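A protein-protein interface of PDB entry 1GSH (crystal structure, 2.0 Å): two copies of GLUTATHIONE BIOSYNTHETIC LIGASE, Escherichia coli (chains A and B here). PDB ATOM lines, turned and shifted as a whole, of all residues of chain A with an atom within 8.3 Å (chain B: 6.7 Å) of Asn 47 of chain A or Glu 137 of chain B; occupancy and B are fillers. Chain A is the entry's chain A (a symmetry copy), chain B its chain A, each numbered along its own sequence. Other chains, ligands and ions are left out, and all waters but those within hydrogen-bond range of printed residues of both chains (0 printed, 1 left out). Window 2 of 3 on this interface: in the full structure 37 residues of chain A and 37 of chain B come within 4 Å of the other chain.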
ATOM      1  N   TYR A  44     -16.107 -29.248   2.948  1.00  0.00           N
ATOM      2  CA  TYR A  44     -16.693 -28.074   3.533  1.00  0.00           C
ATOM      3  C   TYR A  44     -15.779 -26.927   3.250  1.00  0.00           C
ATOM      4  O   TYR A  44     -14.692 -27.095   2.706  1.00  0.00           O
ATOM      5  CB  TYR A  44     -16.901 -28.306   5.041  1.00  0.00           C
ATOM      6  CG  TYR A  44     -15.655 -28.516   5.881  1.00  0.00           C
ATOM      7  CD1 TYR A  44     -15.023 -29.762   5.981  1.00  0.00           C
ATOM      8  CD2 TYR A  44     -15.190 -27.414   6.582  1.00  0.00           C
ATOM      9  CE1 TYR A  44     -13.909 -29.904   6.798  1.00  0.00           C
ATOM     10  CE2 TYR A  44     -14.086 -27.543   7.397  1.00  0.00           C
ATOM     11  CZ  TYR A  44     -13.458 -28.779   7.501  1.00  0.00           C
ATOM     12  OH  TYR A  44     -12.392 -28.861   8.375  1.00  0.00           O
ATOM     13  N   LEU A  45     -16.210 -25.761   3.683  1.00  0.00           N
ATOM     14  CA  LEU A  45     -15.479 -24.548   3.363  1.00  0.00           C
ATOM     15  C   LEU A  45     -15.422 -23.739   4.639  1.00  0.00           C
ATOM     16  O   LEU A  45     -16.459 -23.538   5.243  1.00  0.00           O
ATOM     17  CB  LEU A  45     -16.261 -23.844   2.259  1.00  0.00           C
ATOM     18  CG  LEU A  45     -15.675 -22.919   1.223  1.00  0.00           C
ATOM     19  CD1 LEU A  45     -14.551 -23.566   0.447  1.00  0.00           C
ATOM     20  CD2 LEU A  45     -16.798 -22.587   0.235  1.00  0.00           C
ATOM     21  N   ILE A  46     -14.248 -23.315   5.107  1.00  0.00           N
ATOM     22  CA  ILE A  46     -14.135 -22.508   6.310  1.00  0.00           C
ATOM     23  C   ILE A  46     -13.234 -21.339   5.953  1.00  0.00           C
ATOM     24  O   ILE A  46     -12.084 -21.486   5.547  1.00  0.00           O
ATOM     25  CB  ILE A  46     -13.582 -23.401   7.525  1.00  0.00           C
ATOM     26  CG1 ILE A  46     -13.382 -22.501   8.765  1.00  0.00           C
ATOM     27  CG2 ILE A  46     -12.279 -24.145   7.169  1.00  0.00           C
ATOM     28  CD1 ILE A  46     -14.656 -21.861   9.414  1.00  0.00           C
ATOM     29  N   ASN A  47     -13.847 -20.161   6.050  1.00  0.00           N
ATOM     30  CA  ASN A  47     -13.247 -18.875   5.705  1.00  0.00           C
ATOM     31  C   ASN A  47     -12.513 -18.918   4.374  1.00  0.00           C
ATOM     32  O   ASN A  47     -11.354 -18.531   4.239  1.00  0.00           O
ATOM     33  CB  ASN A  47     -12.286 -18.417   6.804  1.00  0.00           C
ATOM     34  CG  ASN A  47     -13.002 -18.174   8.123  1.00  0.00           C
ATOM     35  OD1 ASN A  47     -14.124 -17.687   8.190  1.00  0.00           O
ATOM     36  ND2 ASN A  47     -12.399 -18.550   9.232  1.00  0.00           N
ATOM     37  N   GLY A  48     -13.197 -19.499   3.393  1.00  0.00           N
ATOM     38  CA  GLY A  48     -12.680 -19.523   2.043  1.00  0.00           C
ATOM     39  C   GLY A  48     -11.722 -20.669   1.782  1.00  0.00           C
ATOM     40  O   GLY A  48     -11.306 -20.845   0.648  1.00  0.00           O
ATOM     41  N   GLU A  49     -11.330 -21.459   2.777  1.00  0.00           N
ATOM     42  CA  GLU A  49     -10.413 -22.545   2.550  1.00  0.00           C
ATOM     43  C   GLU A  49     -11.216 -23.815   2.374  1.00  0.00           C
ATOM     44  O   GLU A  49     -12.152 -24.074   3.110  1.00  0.00           O
ATOM     45  CB  GLU A  49      -9.466 -22.681   3.734  1.00  0.00           C
ATOM     46  CG  GLU A  49      -8.512 -23.863   3.628  1.00  0.00           C
ATOM     47  CD  GLU A  49      -7.549 -24.051   4.803  1.00  0.00           C
ATOM     48  OE1 GLU A  49      -7.962 -24.073   5.977  1.00  0.00           O
ATOM     49  OE2 GLU A  49      -6.361 -24.188   4.514  1.00  0.00           O
ATOM     50  N   ALA A  50     -10.858 -24.632   1.386  1.00  0.00           N
ATOM     51  CA  ALA A  50     -11.552 -25.861   1.119  1.00  0.00           C
ATOM     52  C   ALA A  50     -10.865 -26.936   1.943  1.00  0.00           C
ATOM     53  O   ALA A  50      -9.640 -27.035   1.999  1.00  0.00           O
ATOM     54  CB  ALA A  50     -11.445 -26.155  -0.353  1.00  0.00           C
ATOM     55  N   ARG A  51     -11.682 -27.730   2.609  1.00  0.00           N
ATOM     56  CA  ARG A  51     -11.204 -28.803   3.464  1.00  0.00           C
ATOM     57  C   ARG A  51     -12.117 -29.983   3.377  1.00  0.00           C
ATOM     58  O   ARG A  51     -13.263 -29.886   2.931  1.00  0.00           O
ATOM     59  CB  ARG A  51     -11.191 -28.437   4.911  1.00  0.00           C
ATOM     60  CG  ARG A  51     -10.290 -27.323   5.312  1.00  0.00           C
ATOM     61  CD  ARG A  51     -10.083 -27.614   6.777  1.00  0.00           C
ATOM     62  NE  ARG A  51      -8.903 -26.905   7.156  1.00  0.00           N
ATOM     63  CZ  ARG A  51      -7.859 -27.503   7.701  1.00  0.00           C
ATOM     64  NH1 ARG A  51      -7.835 -28.794   7.978  1.00  0.00           N
ATOM     65  NH2 ARG A  51      -6.758 -26.764   7.838  1.00  0.00           N
ATOM     66  N   ARG A 104     -11.786 -23.860  -4.952  1.00  0.00           N
ATOM     67  CA  ARG A 104     -10.918 -23.178  -3.993  1.00  0.00           C
ATOM     68  C   ARG A 104      -9.631 -23.976  -3.753  1.00  0.00           C
ATOM     69  O   ARG A 104      -8.569 -23.410  -3.478  1.00  0.00           O
ATOM     70  CB  ARG A 104     -11.671 -23.000  -2.711  1.00  0.00           C
ATOM     71  CG  ARG A 104     -12.863 -22.070  -2.875  1.00  0.00           C
ATOM     72  CD  ARG A 104     -12.534 -20.781  -2.177  1.00  0.00           C
ATOM     73  NE  ARG A 104     -11.695 -19.898  -2.950  1.00  0.00           N
ATOM     74  CZ  ARG A 104     -10.734 -19.103  -2.421  1.00  0.00           C
ATOM     75  NH1 ARG A 104     -10.389 -19.026  -1.146  1.00  0.00           N
ATOM     76  NH2 ARG A 104     -10.144 -18.239  -3.222  1.00  0.00           N
ATOM     77  N   THR B 128     -18.342 -14.928  -1.751  1.00  0.00           N
ATOM     78  CA  THR B 128     -17.634 -14.296  -0.648  1.00  0.00           C
ATOM     79  C   THR B 128     -16.440 -15.142  -0.187  1.00  0.00           C
ATOM     80  O   THR B 128     -15.584 -14.627   0.522  1.00  0.00           O
ATOM     81  CB  THR B 128     -18.600 -14.083   0.509  1.00  0.00           C
ATOM     82  OG1 THR B 128     -18.992 -15.366   0.963  1.00  0.00           O
ATOM     83  CG2 THR B 128     -19.787 -13.224   0.100  1.00  0.00           C
ATOM     84  N   ALA B 129     -16.339 -16.431  -0.573  1.00  0.00           N
ATOM     85  CA  ALA B 129     -15.201 -17.274  -0.253  1.00  0.00           C
ATOM     86  C   ALA B 129     -13.950 -16.749  -0.916  1.00  0.00           C
ATOM     87  O   ALA B 129     -12.859 -17.079  -0.453  1.00  0.00           O
ATOM     88  CB  ALA B 129     -15.377 -18.688  -0.743  1.00  0.00           C
ATOM     89  N   SER B 132     -12.350 -13.567   1.738  1.00  0.00           N
ATOM     90  CA  SER B 132     -12.482 -13.925   3.141  1.00  0.00           C
ATOM     91  C   SER B 132     -11.986 -12.869   4.116  1.00  0.00           C
ATOM     92  O   SER B 132     -12.443 -12.797   5.251  1.00  0.00           O
ATOM     93  CB  SER B 132     -11.755 -15.229   3.389  1.00  0.00           C
ATOM     94  OG  SER B 132     -10.392 -15.109   3.020  1.00  0.00           O
ATOM     95  N   ASP B 133     -11.076 -12.027   3.631  1.00  0.00           N
ATOM     96  CA  ASP B 133     -10.569 -10.850   4.324  1.00  0.00           C
ATOM     97  C   ASP B 133     -11.641  -9.848   4.728  1.00  0.00           C
ATOM     98  O   ASP B 133     -11.486  -9.101   5.698  1.00  0.00           O
ATOM     99  CB  ASP B 133      -9.580 -10.097   3.436  1.00  0.00           C
ATOM    100  CG  ASP B 133      -8.204 -10.736   3.273  1.00  0.00           C
ATOM    101  OD1 ASP B 133      -7.982 -11.848   3.789  1.00  0.00           O
ATOM    102  OD2 ASP B 133      -7.344 -10.108   2.632  1.00  0.00           O
ATOM    103  N   THR B 135     -15.058 -10.721   4.930  1.00  0.00           N
ATOM    104  CA  THR B 135     -16.291 -11.354   5.363  1.00  0.00           C
ATOM    105  C   THR B 135     -16.242 -11.739   6.820  1.00  0.00           C
ATOM    106  O   THR B 135     -15.143 -11.753   7.389  1.00  0.00           O
ATOM    107  CB  THR B 135     -16.569 -12.617   4.512  1.00  0.00           C
ATOM    108  OG1 THR B 135     -15.540 -13.547   4.801  1.00  0.00           O
ATOM    109  CG2 THR B 135     -16.651 -12.312   3.041  1.00  0.00           C
ATOM    110  N   PRO B 136     -17.375 -12.038   7.476  1.00  0.00           N
ATOM    111  CA  PRO B 136     -17.380 -12.688   8.777  1.00  0.00           C
ATOM    112  C   PRO B 136     -16.876 -14.112   8.693  1.00  0.00           C
ATOM    113  O   PRO B 136     -16.578 -14.634   7.620  1.00  0.00           O
ATOM    114  CB  PRO B 136     -18.813 -12.571   9.229  1.00  0.00           C
ATOM    115  CG  PRO B 136     -19.611 -12.433   7.949  1.00  0.00           C
ATOM    116  CD  PRO B 136     -18.712 -11.592   7.093  1.00  0.00           C
ATOM    117  N   GLU B 137     -16.774 -14.732   9.858  1.00  0.00           N
ATOM    118  CA  GLU B 137     -16.384 -16.130   9.963  1.00  0.00           C
ATOM    119  C   GLU B 137     -17.459 -16.876   9.222  1.00  0.00           C
ATOM    120  O   GLU B 137     -18.613 -16.679   9.545  1.00  0.00           O
ATOM    121  CB  GLU B 137     -16.389 -16.590  11.405  1.00  0.00           C
ATOM    122  CG  GLU B 137     -15.382 -15.847  12.255  1.00  0.00           C
ATOM    123  CD  GLU B 137     -13.981 -16.168  11.809  1.00  0.00           C
ATOM    124  OE1 GLU B 137     -13.535 -17.310  11.991  1.00  0.00           O
ATOM    125  OE2 GLU B 137     -13.357 -15.256  11.269  1.00  0.00           O
ATOM    126  N   THR B 138     -17.113 -17.648   8.215  1.00  0.00           N
ATOM    127  CA  THR B 138     -18.099 -18.348   7.447  1.00  0.00           C
ATOM    128  C   THR B 138     -17.759 -19.802   7.347  1.00  0.00           C
ATOM    129  O   THR B 138     -16.642 -20.141   6.986  1.00  0.00           O
ATOM    130  CB  THR B 138     -18.169 -17.770   6.073  1.00  0.00           C
ATOM    131  OG1 THR B 138     -18.433 -16.390   6.239  1.00  0.00           O
ATOM    132  CG2 THR B 138     -19.269 -18.391   5.226  1.00  0.00           C
ATOM    133  N   LEU B 139     -18.733 -20.651   7.672  1.00  0.00           N
ATOM    134  CA  LEU B 139     -18.588 -22.092   7.500  1.00  0.00           C
ATOM    135  C   LEU B 139     -19.648 -22.625   6.533  1.00  0.00           C
ATOM    136  O   LEU B 139     -20.816 -22.292   6.709  1.00  0.00           O
ATOM    137  CB  LEU B 139     -18.738 -22.806   8.867  1.00  0.00           C
ATOM    138  CG  LEU B 139     -18.908 -24.340   8.916  1.00  0.00           C
ATOM    139  CD1 LEU B 139     -17.669 -25.065   8.351  1.00  0.00           C
ATOM    140  CD2 LEU B 139     -19.193 -24.723  10.359  1.00  0.00           C
ATOM    141  N   VAL B 140     -19.321 -23.446   5.518  1.00  0.00           N
ATOM    142  CA  VAL B 140     -20.318 -24.061   4.638  1.00  0.00           C
ATOM    143  C   VAL B 140     -20.219 -25.563   4.827  1.00  0.00           C
ATOM    144  O   VAL B 140     -19.182 -26.158   4.523  1.00  0.00           O
ATOM    145  CB  VAL B 140     -20.046 -23.708   3.158  1.00  0.00           C
ATOM    146  CG1 VAL B 140     -21.106 -24.284   2.236  1.00  0.00           C
ATOM    147  CG2 VAL B 140     -20.125 -22.187   3.011  1.00  0.00           C
ATOM    148  N   PHE B 150     -18.918 -24.693  15.578  1.00  0.00           N
ATOM    149  CA  PHE B 150     -18.836 -23.289  15.217  1.00  0.00           C
ATOM    150  C   PHE B 150     -19.670 -22.460  16.183  1.00  0.00           C
ATOM    151  O   PHE B 150     -19.289 -21.339  16.500  1.00  0.00           O
ATOM    152  CB  PHE B 150     -19.362 -23.138  13.789  1.00  0.00           C
ATOM    153  CG  PHE B 150     -19.134 -21.798  13.095  1.00  0.00           C
ATOM    154  CD1 PHE B 150     -17.896 -21.503  12.526  1.00  0.00           C
ATOM    155  CD2 PHE B 150     -20.187 -20.870  13.006  1.00  0.00           C
ATOM    156  CE1 PHE B 150     -17.715 -20.285  11.865  1.00  0.00           C
ATOM    157  CE2 PHE B 150     -19.985 -19.658  12.345  1.00  0.00           C
ATOM    158  CZ  PHE B 150     -18.755 -19.359  11.781  1.00  0.00           C
ATOM    159  N   LYS B 153     -17.803 -22.125  19.431  1.00  0.00           N
ATOM    160  CA  LYS B 153     -16.692 -21.208  19.339  1.00  0.00           C
ATOM    161  C   LYS B 153     -17.155 -19.774  19.280  1.00  0.00           C
ATOM    162  O   LYS B 153     -16.483 -18.892  19.803  1.00  0.00           O
ATOM    163  CB  LYS B 153     -15.874 -21.555  18.107  1.00  0.00           C
ATOM    164  CG  LYS B 153     -14.790 -20.535  17.833  1.00  0.00           C
ATOM    165  CD  LYS B 153     -14.042 -20.761  16.540  1.00  0.00           C
ATOM    166  CE  LYS B 153     -13.141 -19.530  16.373  1.00  0.00           C
ATOM    167  NZ  LYS B 153     -12.156 -19.688  15.317  1.00  0.00           N
ATOM    168  N   HIS B 154     -18.299 -19.508  18.653  1.00  0.00           N
ATOM    169  CA  HIS B 154     -18.740 -18.140  18.467  1.00  0.00           C
ATOM    170  C   HIS B 154     -19.902 -17.671  19.320  1.00  0.00           C
ATOM    171  O   HIS B 154     -20.195 -16.472  19.310  1.00  0.00           O
ATOM    172  CB  HIS B 154     -19.078 -17.932  16.993  1.00  0.00           C
ATOM    173  CG  HIS B 154     -17.810 -17.907  16.171  1.00  0.00           C
ATOM    174  ND1 HIS B 154     -16.871 -16.960  16.173  1.00  0.00           N
ATOM    175  CD2 HIS B 154     -17.417 -18.900  15.313  1.00  0.00           C
ATOM    176  CE1 HIS B 154     -15.929 -17.347  15.355  1.00  0.00           C
ATOM    177  NE2 HIS B 154     -16.265 -18.507  14.846  1.00  0.00           N
ATOM    178  N   ALA B 197     -23.124 -21.069   7.871  1.00  0.00           N
ATOM    179  CA  ALA B 197     -23.182 -20.432   9.177  1.00  0.00           C
ATOM    180  C   ALA B 197     -22.200 -19.268   9.175  1.00  0.00           C
ATOM    181  O   ALA B 197     -21.145 -19.377   8.564  1.00  0.00           O
ATOM    182  CB  ALA B 197     -22.763 -21.390  10.300  1.00  0.00           C
ATOM    183  N   GLN B 198     -22.501 -18.130   9.815  1.00  0.00           N
ATOM    184  CA  GLN B 198     -21.580 -17.013   9.928  1.00  0.00           C
ATOM    185  C   GLN B 198     -21.711 -16.536  11.354  1.00  0.00           C
ATOM    186  O   GLN B 198     -22.731 -16.797  11.974  1.00  0.00           O
ATOM    187  CB  GLN B 198     -21.937 -15.808   9.068  1.00  0.00           C
ATOM    188  CG  GLN B 198     -21.949 -16.134   7.609  1.00  0.00           C
ATOM    189  CD  GLN B 198     -22.318 -14.957   6.761  1.00  0.00           C
ATOM    190  OE1 GLN B 198     -23.343 -14.292   6.938  1.00  0.00           O
ATOM    191  NE2 GLN B 198     -21.445 -14.707   5.800  1.00  0.00           N
ATOM    192  N   ASN B 199     -20.751 -15.834  11.935  1.00  0.00           N
ATOM    193  CA  ASN B 199     -20.969 -15.312  13.283  1.00  0.00           C
ATOM    194  C   ASN B 199     -21.907 -14.122  13.162  1.00  0.00           C
ATOM    195  O   ASN B 199     -21.926 -13.419  12.149  1.00  0.00           O
ATOM    196  CB  ASN B 199     -19.650 -14.889  13.932  1.00  0.00           C
ATOM    197  CG  ASN B 199     -18.867 -13.882  13.138  1.00  0.00           C
ATOM    198  OD1 ASN B 199     -18.540 -14.121  11.982  1.00  0.00           O
ATOM    199  ND2 ASN B 199     -18.536 -12.732  13.709  1.00  0.00           N
ATOM    200  N   ARG B 278     -18.126  -5.497   7.370  1.00  0.00           N
ATOM    201  CA  ARG B 278     -18.148  -6.857   6.859  1.00  0.00           C
ATOM    202  C   ARG B 278     -19.019  -7.018   5.622  1.00  0.00           C
ATOM    203  O   ARG B 278     -20.163  -6.543   5.578  1.00  0.00           O
ATOM    204  CB  ARG B 278     -18.650  -7.758   7.974  1.00  0.00           C
ATOM    205  CG  ARG B 278     -17.581  -8.426   8.834  1.00  0.00           C
ATOM    206  CD  ARG B 278     -16.381  -7.570   9.154  1.00  0.00           C
ATOM    207  NE  ARG B 278     -15.195  -8.330   8.830  1.00  0.00           N
ATOM    208  CZ  ARG B 278     -14.179  -7.854   8.105  1.00  0.00           C
ATOM    209  NH1 ARG B 278     -14.149  -6.619   7.607  1.00  0.00           N
ATOM    210  NH2 ARG B 278     -13.171  -8.679   7.844  1.00  0.00           N
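O of Ala 129 of chain B is in hydrogen-bond range of NH1 of Arg 104 of chain A. The side-chain carboxylate (OE1) of Glu 137 of chain B sits at hydrogen-bond distance from the side-chain amide nitrogen (ND2) of Asn 47 of chain A, at 3.2 Å. N of Asn 47 of chain A lies within hydrogen-bond range of O of Thr 138 of chain B (2.9 Å). O of Leu 45 of chain A lies within hydrogen-bond range of N of Val 140 of chain B (2.9 Å).
The side-chain hydroxyl (OG1) of Thr 138 of chain B lies within hydrogen-bond range of the backbone carbonyl oxygen (O) of Pro 136 of chain B (2.9 Å). The backbone NH (N) of Glu 137 of chain B sits at hydrogen-bond distance from the side-chain amide oxygen (OD1) of Asn 199 of chain B (2.8 Å). The side-chain amide nitrogen (NE2) of Gln 198 of chain B is in hydrogen-bond range of the side-chain hydroxyl (OG1) of Thr 138 of chain B. O of Leu 139 of chain B lies within hydrogen-bond range of N of Ala 197 of chain B (2.9 Å). N of Tyr 44 of chain A is in hydrogen-bond range of O of Arg 51 of chain A, at 2.9 Å. O of Gly 48 of chain A lies within hydrogen-bond range of NH1 of Arg 104 of chain A, at 2.7 Å.
Among the printed residues, pairs that only touch across the chains: Tyr 44 of chain A with Leu 139 of chain B (3.8 Å), Tyr 44 of chain A with Val 140 of chain B (3.2 Å), Leu 45 of chain A with Thr 138 of chain B (3.8 Å), Leu 45 of chain A with Leu 139 of chain B (3.4 Å), Ile 46 of chain A with Thr 138 of chain B (3.5 Å), Asn 47 of chain A with Ser 132 of chain B (3.4 Å), Asn 47 of chain A with Pro 136 of chain B (3.96 Å) and Gly 48 of chain A with Ala 129 of chain B (3.5 Å).
Asn 47 of chain A touches four residues of chain B. Glu 137 of chain B touches just one residue of chain A: Asn 47 (3.2 Å). Of the printed residues of chain A, Ser 132 of chain B touches Asn 47. Printed residues of chain A within 4 Å of Leu 139 of chain B: Tyr 44 and Leu 45. Printed residues of chain B within 4 Å of Leu 45 of chain A: Thr 138, Leu 139 and Val 140.
Of the 9 printed residues of chain A, 6 touch a printed residue of chain B. Hydrophobic or aromatic side chains of chain A within 4 Å of the printed part of chain B: Tyr 44, Leu 45 and Ile 46.
No position is printed for both chains. Of the 12 pairs that touch across the chains among the printed residues, none has its exchanged pair printed and touching as well.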
